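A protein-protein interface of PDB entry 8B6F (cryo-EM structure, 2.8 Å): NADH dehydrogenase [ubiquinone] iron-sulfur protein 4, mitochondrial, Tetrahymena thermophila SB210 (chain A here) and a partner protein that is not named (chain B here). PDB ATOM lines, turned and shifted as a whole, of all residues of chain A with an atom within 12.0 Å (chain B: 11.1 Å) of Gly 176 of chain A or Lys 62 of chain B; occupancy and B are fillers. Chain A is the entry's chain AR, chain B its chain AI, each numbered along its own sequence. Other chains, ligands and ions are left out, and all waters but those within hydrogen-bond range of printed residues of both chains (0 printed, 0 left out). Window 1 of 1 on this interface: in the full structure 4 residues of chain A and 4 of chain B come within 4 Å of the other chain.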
ATOM      1  N   ASN A 171       8.287  -1.434  -1.454  1.00  0.00           N
ATOM      2  CA  ASN A 171       8.774  -1.107  -2.790  1.00  0.00           C
ATOM      3  C   ASN A 171       9.280  -2.353  -3.508  1.00  0.00           C
ATOM      4  O   ASN A 171       9.061  -2.515  -4.714  1.00  0.00           O
ATOM      5  CB  ASN A 171       9.877  -0.051  -2.701  1.00  0.00           C
ATOM      6  CG  ASN A 171       9.383   1.263  -2.126  1.00  0.00           C
ATOM      7  OD1 ASN A 171       8.325   1.321  -1.501  1.00  0.00           O
ATOM      8  ND2 ASN A 171      10.151   2.325  -2.333  1.00  0.00           N
ATOM      9  N   MET A 172       9.958  -3.243  -2.784  1.00  0.00           N
ATOM     10  CA  MET A 172      10.466  -4.495  -3.339  1.00  0.00           C
ATOM     11  C   MET A 172       9.516  -5.621  -2.947  1.00  0.00           C
ATOM     12  O   MET A 172       9.440  -5.996  -1.773  1.00  0.00           O
ATOM     13  CB  MET A 172      11.876  -4.784  -2.834  1.00  0.00           C
ATOM     14  CG  MET A 172      12.910  -3.746  -3.229  1.00  0.00           C
ATOM     15  SD  MET A 172      12.685  -2.154  -2.415  1.00  0.00           S
ATOM     16  CE  MET A 172      13.038  -2.585  -0.711  1.00  0.00           C
ATOM     17  N   LEU A 173       8.798  -6.161  -3.930  1.00  0.00           N
ATOM     18  CA  LEU A 173       7.882  -7.272  -3.715  1.00  0.00           C
ATOM     19  C   LEU A 173       8.102  -8.324  -4.790  1.00  0.00           C
ATOM     20  O   LEU A 173       8.262  -7.994  -5.969  1.00  0.00           O
ATOM     21  CB  LEU A 173       6.421  -6.803  -3.734  1.00  0.00           C
ATOM     22  CG  LEU A 173       6.013  -5.829  -2.626  1.00  0.00           C
ATOM     23  CD1 LEU A 173       4.596  -5.332  -2.853  1.00  0.00           C
ATOM     24  CD2 LEU A 173       6.138  -6.475  -1.253  1.00  0.00           C
ATOM     25  N   TRP A 174       8.107  -9.585  -4.380  1.00  0.00           N
ATOM     26  CA  TRP A 174       8.294 -10.683  -5.319  1.00  0.00           C
ATOM     27  C   TRP A 174       6.980 -10.968  -6.039  1.00  0.00           C
ATOM     28  O   TRP A 174       5.996 -11.330  -5.384  1.00  0.00           O
ATOM     29  CB  TRP A 174       8.777 -11.923  -4.584  1.00  0.00           C
ATOM     30  CG  TRP A 174       8.864 -13.148  -5.434  1.00  0.00           C
ATOM     31  CD1 TRP A 174       9.640 -13.324  -6.541  1.00  0.00           C
ATOM     32  CD2 TRP A 174       8.158 -14.378  -5.238  1.00  0.00           C
ATOM     33  NE1 TRP A 174       9.459 -14.588  -7.048  1.00  0.00           N
ATOM     34  CE2 TRP A 174       8.553 -15.255  -6.266  1.00  0.00           C
ATOM     35  CE3 TRP A 174       7.230 -14.821  -4.291  1.00  0.00           C
ATOM     36  CZ2 TRP A 174       8.051 -16.549  -6.376  1.00  0.00           C
ATOM     37  CZ3 TRP A 174       6.732 -16.105  -4.401  1.00  0.00           C
ATOM     38  CH2 TRP A 174       7.143 -16.956  -5.437  1.00  0.00           C
ATOM     39  N   PRO A 175       6.915 -10.822  -7.366  1.00  0.00           N
ATOM     40  CA  PRO A 175       5.618 -11.004  -8.043  1.00  0.00           C
ATOM     41  C   PRO A 175       5.037 -12.396  -7.881  1.00  0.00           C
ATOM     42  O   PRO A 175       3.812 -12.542  -7.785  1.00  0.00           O
ATOM     43  CB  PRO A 175       5.946 -10.688  -9.509  1.00  0.00           C
ATOM     44  CG  PRO A 175       7.401 -10.943  -9.639  1.00  0.00           C
ATOM     45  CD  PRO A 175       8.002 -10.557  -8.324  1.00  0.00           C
ATOM     46  N   GLY A 176       5.877 -13.424  -7.851  1.00  0.00           N
ATOM     47  CA  GLY A 176       5.436 -14.798  -7.762  1.00  0.00           C
ATOM     48  C   GLY A 176       6.059 -15.651  -8.843  1.00  0.00           C
ATOM     49  O   GLY A 176       6.837 -15.186  -9.675  1.00  0.00           O
ATOM     50  N   HIS A 177       5.700 -16.932  -8.822  1.00  0.00           N
ATOM     51  CA  HIS A 177       6.212 -17.861  -9.819  1.00  0.00           C
ATOM     52  C   HIS A 177       5.720 -17.476 -11.207  1.00  0.00           C
ATOM     53  O   HIS A 177       4.585 -17.025 -11.381  1.00  0.00           O
ATOM     54  CB  HIS A 177       5.785 -19.291  -9.487  1.00  0.00           C
ATOM     55  CG  HIS A 177       6.512 -19.882  -8.320  1.00  0.00           C
ATOM     56  ND1 HIS A 177       6.146 -19.640  -7.012  1.00  0.00           N
ATOM     57  CD2 HIS A 177       7.587 -20.702  -8.262  1.00  0.00           C
ATOM     58  CE1 HIS A 177       6.963 -20.288  -6.201  1.00  0.00           C
ATOM     59  NE2 HIS A 177       7.847 -20.940  -6.935  1.00  0.00           N
ATOM     60  N   ASP A 178       6.590 -17.655 -12.204  1.00  0.00           N
ATOM     61  CA  ASP A 178       6.222 -17.310 -13.573  1.00  0.00           C
ATOM     62  C   ASP A 178       5.060 -18.162 -14.066  1.00  0.00           C
ATOM     63  O   ASP A 178       4.146 -17.658 -14.728  1.00  0.00           O
ATOM     64  CB  ASP A 178       7.431 -17.469 -14.493  1.00  0.00           C
ATOM     65  CG  ASP A 178       8.593 -16.583 -14.087  1.00  0.00           C
ATOM     66  OD1 ASP A 178       8.455 -15.845 -13.090  1.00  0.00           O
ATOM     67  OD2 ASP A 178       9.642 -16.626 -14.762  1.00  0.00           O
ATOM     68  N   ASN A 179       5.077 -19.459 -13.752  1.00  0.00           N
ATOM     69  CA  ASN A 179       4.021 -20.359 -14.198  1.00  0.00           C
ATOM     70  C   ASN A 179       2.683 -20.081 -13.526  1.00  0.00           C
ATOM     71  O   ASN A 179       1.661 -20.597 -13.990  1.00  0.00           O
ATOM     72  CB  ASN A 179       4.430 -21.809 -13.938  1.00  0.00           C
ATOM     73  CG  ASN A 179       4.661 -22.094 -12.465  1.00  0.00           C
ATOM     74  OD1 ASN A 179       5.778 -21.962 -11.963  1.00  0.00           O
ATOM     75  ND2 ASN A 179       3.603 -22.484 -11.765  1.00  0.00           N
ATOM     76  N   ALA A 180       2.663 -19.293 -12.454  1.00  0.00           N
ATOM     77  CA  ALA A 180       1.416 -19.018 -11.755  1.00  0.00           C
ATOM     78  C   ALA A 180       0.411 -18.355 -12.689  1.00  0.00           C
ATOM     79  O   ALA A 180       0.761 -17.487 -13.492  1.00  0.00           O
ATOM     80  CB  ALA A 180       1.675 -18.124 -10.542  1.00  0.00           C
ATOM     81  N   VAL A 181      -0.846 -18.773 -12.578  1.00  0.00           N
ATOM     82  CA  VAL A 181      -1.923 -18.208 -13.382  1.00  0.00           C
ATOM     83  C   VAL A 181      -3.076 -17.787 -12.480  1.00  0.00           C
ATOM     84  O   VAL A 181      -2.934 -17.747 -11.257  1.00  0.00           O
ATOM     85  CB  VAL A 181      -2.407 -19.205 -14.453  1.00  0.00           C
ATOM     86  CG1 VAL A 181      -1.301 -19.485 -15.458  1.00  0.00           C
ATOM     87  CG2 VAL A 181      -2.884 -20.499 -13.804  1.00  0.00           C
ATOM     88  N   ILE B  55      18.581 -13.881 -24.492  1.00  0.00           N
ATOM     89  CA  ILE B  55      18.661 -13.009 -23.323  1.00  0.00           C
ATOM     90  C   ILE B  55      17.428 -13.178 -22.446  1.00  0.00           C
ATOM     91  O   ILE B  55      17.529 -13.273 -21.218  1.00  0.00           O
ATOM     92  CB  ILE B  55      18.845 -11.546 -23.770  1.00  0.00           C
ATOM     93  CG1 ILE B  55      20.186 -11.378 -24.482  1.00  0.00           C
ATOM     94  CG2 ILE B  55      18.773 -10.602 -22.576  1.00  0.00           C
ATOM     95  CD1 ILE B  55      20.245 -10.170 -25.382  1.00  0.00           C
ATOM     96  N   LEU B  56      16.245 -13.221 -23.061  1.00  0.00           N
ATOM     97  CA  LEU B  56      15.019 -13.414 -22.293  1.00  0.00           C
ATOM     98  C   LEU B  56      15.019 -14.766 -21.593  1.00  0.00           C
ATOM     99  O   LEU B  56      14.576 -14.878 -20.444  1.00  0.00           O
ATOM    100  CB  LEU B  56      13.800 -13.279 -23.205  1.00  0.00           C
ATOM    101  CG  LEU B  56      13.566 -11.893 -23.813  1.00  0.00           C
ATOM    102  CD1 LEU B  56      12.407 -11.935 -24.795  1.00  0.00           C
ATOM    103  CD2 LEU B  56      13.310 -10.853 -22.733  1.00  0.00           C
ATOM    104  N   ALA B  57      15.511 -15.804 -22.268  1.00  0.00           N
ATOM    105  CA  ALA B  57      15.609 -17.115 -21.636  1.00  0.00           C
ATOM    106  C   ALA B  57      16.549 -17.078 -20.440  1.00  0.00           C
ATOM    107  O   ALA B  57      16.266 -17.682 -19.398  1.00  0.00           O
ATOM    108  CB  ALA B  57      16.078 -18.155 -22.655  1.00  0.00           C
ATOM    109  N   LYS B  58      17.676 -16.376 -20.567  1.00  0.00           N
ATOM    110  CA  LYS B  58      18.587 -16.238 -19.436  1.00  0.00           C
ATOM    111  C   LYS B  58      17.906 -15.547 -18.262  1.00  0.00           C
ATOM    112  O   LYS B  58      18.046 -15.978 -17.111  1.00  0.00           O
ATOM    113  CB  LYS B  58      19.834 -15.461 -19.860  1.00  0.00           C
ATOM    114  CG  LYS B  58      20.742 -16.212 -20.822  1.00  0.00           C
ATOM    115  CD  LYS B  58      21.891 -15.332 -21.295  1.00  0.00           C
ATOM    116  CE  LYS B  58      22.758 -16.058 -22.312  1.00  0.00           C
ATOM    117  NZ  LYS B  58      23.857 -15.193 -22.824  1.00  0.00           N
ATOM    118  N   TYR B  59      17.172 -14.474 -18.526  1.00  0.00           N
ATOM    119  CA  TYR B  59      16.457 -13.770 -17.476  1.00  0.00           C
ATOM    120  C   TYR B  59      15.158 -14.492 -17.132  1.00  0.00           C
ATOM    121  O   TYR B  59      14.666 -15.313 -17.908  1.00  0.00           O
ATOM    122  CB  TYR B  59      16.161 -12.339 -17.912  1.00  0.00           C
ATOM    123  CG  TYR B  59      17.385 -11.455 -17.940  1.00  0.00           C
ATOM    124  CD1 TYR B  59      17.975 -11.014 -16.764  1.00  0.00           C
ATOM    125  CD2 TYR B  59      17.947 -11.057 -19.146  1.00  0.00           C
ATOM    126  CE1 TYR B  59      19.094 -10.206 -16.785  1.00  0.00           C
ATOM    127  CE2 TYR B  59      19.066 -10.248 -19.178  1.00  0.00           C
ATOM    128  CZ  TYR B  59      19.635  -9.826 -17.995  1.00  0.00           C
ATOM    129  OH  TYR B  59      20.748  -9.021 -18.025  1.00  0.00           O
ATOM    130  N   PRO B  60      14.580 -14.206 -15.965  1.00  0.00           N
ATOM    131  CA  PRO B  60      13.316 -14.852 -15.598  1.00  0.00           C
ATOM    132  C   PRO B  60      12.216 -14.524 -16.596  1.00  0.00           C
ATOM    133  O   PRO B  60      12.193 -13.451 -17.200  1.00  0.00           O
ATOM    134  CB  PRO B  60      13.004 -14.272 -14.213  1.00  0.00           C
ATOM    135  CG  PRO B  60      14.304 -13.787 -13.695  1.00  0.00           C
ATOM    136  CD  PRO B  60      15.082 -13.332 -14.892  1.00  0.00           C
ATOM    137  N   LEU B  61      11.295 -15.474 -16.764  1.00  0.00           N
ATOM    138  CA  LEU B  61      10.220 -15.297 -17.736  1.00  0.00           C
ATOM    139  C   LEU B  61       9.386 -14.066 -17.412  1.00  0.00           C
ATOM    140  O   LEU B  61       9.074 -13.266 -18.302  1.00  0.00           O
ATOM    141  CB  LEU B  61       9.343 -16.551 -17.776  1.00  0.00           C
ATOM    142  CG  LEU B  61       8.434 -16.774 -18.993  1.00  0.00           C
ATOM    143  CD1 LEU B  61       7.852 -18.177 -18.958  1.00  0.00           C
ATOM    144  CD2 LEU B  61       7.308 -15.752 -19.092  1.00  0.00           C
ATOM    145  N   LYS B  62       9.033 -13.882 -16.140  1.00  0.00           N
ATOM    146  CA  LYS B  62       8.198 -12.746 -15.769  1.00  0.00           C
ATOM    147  C   LYS B  62       8.991 -11.446 -15.788  1.00  0.00           C
ATOM    148  O   LYS B  62       8.474 -10.405 -16.209  1.00  0.00           O
ATOM    149  CB  LYS B  62       7.585 -12.980 -14.389  1.00  0.00           C
ATOM    150  CG  LYS B  62       6.618 -11.892 -13.956  1.00  0.00           C
ATOM    151  CD  LYS B  62       6.042 -12.164 -12.575  1.00  0.00           C
ATOM    152  CE  LYS B  62       5.102 -13.362 -12.563  1.00  0.00           C
ATOM    153  NZ  LYS B  62       3.934 -13.176 -13.469  1.00  0.00           N
ATOM    154  N   GLN B  63      10.244 -11.482 -15.341  1.00  0.00           N
ATOM    155  CA  GLN B  63      11.061 -10.274 -15.228  1.00  0.00           C
ATOM    156  C   GLN B  63      11.744  -9.955 -16.560  1.00  0.00           C
ATOM    157  O   GLN B  63      12.969  -9.926 -16.679  1.00  0.00           O
ATOM    158  CB  GLN B  63      12.087 -10.438 -14.113  1.00  0.00           C
ATOM    159  CG  GLN B  63      11.484 -10.589 -12.726  1.00  0.00           C
ATOM    160  CD  GLN B  63      10.868  -9.303 -12.210  1.00  0.00           C
ATOM    161  OE1 GLN B  63      10.807  -8.302 -12.920  1.00  0.00           O
ATOM    162  NE2 GLN B  63      10.412  -9.327 -10.964  1.00  0.00           N
ATOM    163  N   LYS B  64      10.920  -9.708 -17.580  1.00  0.00           N
ATOM    164  CA  LYS B  64      11.440  -9.285 -18.875  1.00  0.00           C
ATOM    165  C   LYS B  64      11.988  -7.867 -18.846  1.00  0.00           C
ATOM    166  O   LYS B  64      12.686  -7.470 -19.784  1.00  0.00           O
ATOM    167  CB  LYS B  64      10.351  -9.382 -19.946  1.00  0.00           C
ATOM    168  CG  LYS B  64       9.816 -10.790 -20.163  1.00  0.00           C
ATOM    169  CD  LYS B  64       8.794 -10.842 -21.293  1.00  0.00           C
ATOM    170  CE  LYS B  64       9.441 -10.603 -22.651  1.00  0.00           C
ATOM    171  NZ  LYS B  64       8.465 -10.746 -23.769  1.00  0.00           N
ATOM    172  N   ARG B  65      11.692  -7.100 -17.795  1.00  0.00           N
ATOM    173  CA  ARG B  65      12.159  -5.726 -17.684  1.00  0.00           C
ATOM    174  C   ARG B  65      13.668  -5.628 -17.508  1.00  0.00           C
ATOM    175  O   ARG B  65      14.220  -4.535 -17.663  1.00  0.00           O
ATOM    176  CB  ARG B  65      11.456  -5.047 -16.508  1.00  0.00           C
ATOM    177  CG  ARG B  65      11.560  -3.533 -16.498  1.00  0.00           C
ATOM    178  CD  ARG B  65      11.014  -2.965 -15.198  1.00  0.00           C
ATOM    179  NE  ARG B  65      10.994  -1.507 -15.198  1.00  0.00           N
ATOM    180  CZ  ARG B  65      12.070  -0.744 -15.076  1.00  0.00           C
ATOM    181  NH1 ARG B  65      13.283  -1.265 -14.988  1.00  0.00           N
ATOM    182  NH2 ARG B  65      11.927   0.578 -15.041  1.00  0.00           N
ATOM    183  N   SER B  66      14.345  -6.730 -17.186  1.00  0.00           N
ATOM    184  CA  SER B  66      15.780  -6.704 -16.940  1.00  0.00           C
ATOM    185  C   SER B  66      16.609  -6.727 -18.217  1.00  0.00           C
ATOM    186  O   SER B  66      17.829  -6.547 -18.142  1.00  0.00           O
ATOM    187  CB  SER B  66      16.183  -7.893 -16.064  1.00  0.00           C
ATOM    188  OG  SER B  66      15.478  -7.886 -14.835  1.00  0.00           O
ATOM    189  N   ALA B  67      15.988  -6.938 -19.376  1.00  0.00           N
ATOM    190  CA  ALA B  67      16.709  -7.080 -20.632  1.00  0.00           C
ATOM    191  C   ALA B  67      16.857  -5.762 -21.383  1.00  0.00           C
ATOM    192  O   ALA B  67      17.116  -5.777 -22.591  1.00  0.00           O
ATOM    193  CB  ALA B  67      16.013  -8.112 -21.520  1.00  0.00           C
ATOM    194  N   VAL B  68      16.705  -4.627 -20.703  1.00  0.00           N
ATOM    195  CA  VAL B  68      16.834  -3.341 -21.382  1.00  0.00           C
ATOM    196  C   VAL B  68      18.272  -3.125 -21.839  1.00  0.00           C
ATOM    197  O   VAL B  68      18.526  -2.772 -22.995  1.00  0.00           O
ATOM    198  CB  VAL B  68      16.360  -2.200 -20.465  1.00  0.00           C
ATOM    199  CG1 VAL B  68      16.507  -0.854 -21.165  1.00  0.00           C
ATOM    200  CG2 VAL B  68      14.928  -2.421 -20.045  1.00  0.00           C
ATOM    201  N   LEU B  94       8.733  -4.299 -27.165  1.00  0.00           N
ATOM    202  CA  LEU B  94       9.073  -5.718 -27.089  1.00  0.00           C
ATOM    203  C   LEU B  94       9.120  -6.204 -25.646  1.00  0.00           C
ATOM    204  O   LEU B  94       8.723  -7.339 -25.357  1.00  0.00           O
ATOM    205  CB  LEU B  94      10.414  -5.975 -27.779  1.00  0.00           C
ATOM    206  CG  LEU B  94      10.461  -5.772 -29.296  1.00  0.00           C
ATOM    207  CD1 LEU B  94      11.856  -6.055 -29.831  1.00  0.00           C
ATOM    208  CD2 LEU B  94       9.435  -6.639 -30.007  1.00  0.00           C
ATOM    209  N   LEU B  95       9.609  -5.372 -24.731  1.00  0.00           N
ATOM    210  CA  LEU B  95       9.728  -5.747 -23.329  1.00  0.00           C
ATOM    211  C   LEU B  95       8.463  -5.474 -22.528  1.00  0.00           C
ATOM    212  O   LEU B  95       8.433  -5.767 -21.329  1.00  0.00           O
ATOM    213  CB  LEU B  95      10.913  -5.011 -22.691  1.00  0.00           C
ATOM    214  CG  LEU B  95      12.287  -5.318 -23.294  1.00  0.00           C
ATOM    215  CD1 LEU B  95      13.358  -4.451 -22.655  1.00  0.00           C
ATOM    216  CD2 LEU B  95      12.638  -6.790 -23.150  1.00  0.00           C
ATOM    217  N   GLU B  96       7.422  -4.921 -23.151  1.00  0.00           N
ATOM    218  CA  GLU B  96       6.150  -4.671 -22.473  1.00  0.00           C
ATOM    219  C   GLU B  96       6.350  -3.797 -21.238  1.00  0.00           C
ATOM    220  O   GLU B  96       5.774  -4.046 -20.178  1.00  0.00           O
ATOM    221  CB  GLU B  96       5.448  -5.980 -22.103  1.00  0.00           C
ATOM    222  CG  GLU B  96       4.899  -6.752 -23.294  1.00  0.00           C
ATOM    223  CD  GLU B  96       5.980  -7.443 -24.097  1.00  0.00           C
ATOM    224  OE1 GLU B  96       7.018  -7.810 -23.508  1.00  0.00           O
ATOM    225  OE2 GLU B  96       5.792  -7.621 -25.319  1.00  0.00           O
ATOM    226  N   MET B  97       7.168  -2.766 -21.377  1.00  0.00           N
ATOM    227  CA  MET B  97       7.474  -1.832 -20.307  1.00  0.00           C
ATOM    228  C   MET B  97       7.309  -0.412 -20.820  1.00  0.00           C
ATOM    229  O   MET B  97       7.364  -0.170 -22.032  1.00  0.00           O
ATOM    230  CB  MET B  97       8.902  -2.035 -19.783  1.00  0.00           C
ATOM    231  CG  MET B  97       9.978  -1.832 -20.837  1.00  0.00           C
ATOM    232  SD  MET B  97      11.614  -2.291 -20.245  1.00  0.00           S
ATOM    233  CE  MET B  97      11.866  -1.068 -18.962  1.00  0.00           C
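The side-chain carboxylate (OD2) of Asp 178 of chain A sits at hydrogen-bond distance from the backbone NH (N) of Leu 61 of chain B.
The backbone NH (N) of Lys 62 of chain B lies within hydrogen-bond range of the side-chain carboxylate (OD2) of Asp 178 of chain A (3.1 Å).
Among the printed residues, pairs that only touch across the chains: Pro 175 of chain A with Lys 62 of chain B (3.4 Å), Pro 175 of chain A with Gln 63 of chain B (3.7 Å), Asp 178 of chain A with Pro 60 of chain B (3.8 Å), Gly 176 of chain A with Lys 62 of chain B (3.8 Å) and His 177 of chain A with Lys 62 of chain B (3.9 Å).
Pro 175 of chain A touches two residues of chain B.
His 177 of chain A touches just one residue of chain B: Lys 62.
Of chain B, only Pro 60, Leu 61 and Lys 62 come within 4 Å of Asp 178 of chain A.
No residue of chain B comes within 4 Å of Ala 180 of chain A.
Pro 60 of chain B touches one residue of chain A.
Of chain A, only Pro 175, Gly 176, His 177 and Asp 178 come within 4 Å of Lys 62 of chain B.
Of chain A, only Pro 175 comes within 4 Å of Gln 63 of chain B.
No residue of chain A comes within 4 Å of Lys 64 of chain B.
The nearest residue of chain B that does not touch Gly 176 of chain A is Gln 63 of chain B (6.9 Å).
The nearest residue of chain A that does not touch Lys 62 of chain B is Ala 180 of chain A (5.4 Å).
Printed residues of chain A that touch a printed residue of chain B: Pro 175, Gly 176, His 177 and Asp 178.
Hydrophobic or aromatic side chains of chain A that line the printed part of chain B: Pro 175.
Among the printed residues, 7 pairs touch across the chains.
Among the printed residues, no Asp or Glu carboxylate lies within 4 Å of a Lys or Arg side-chain nitrogen of the other chain.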
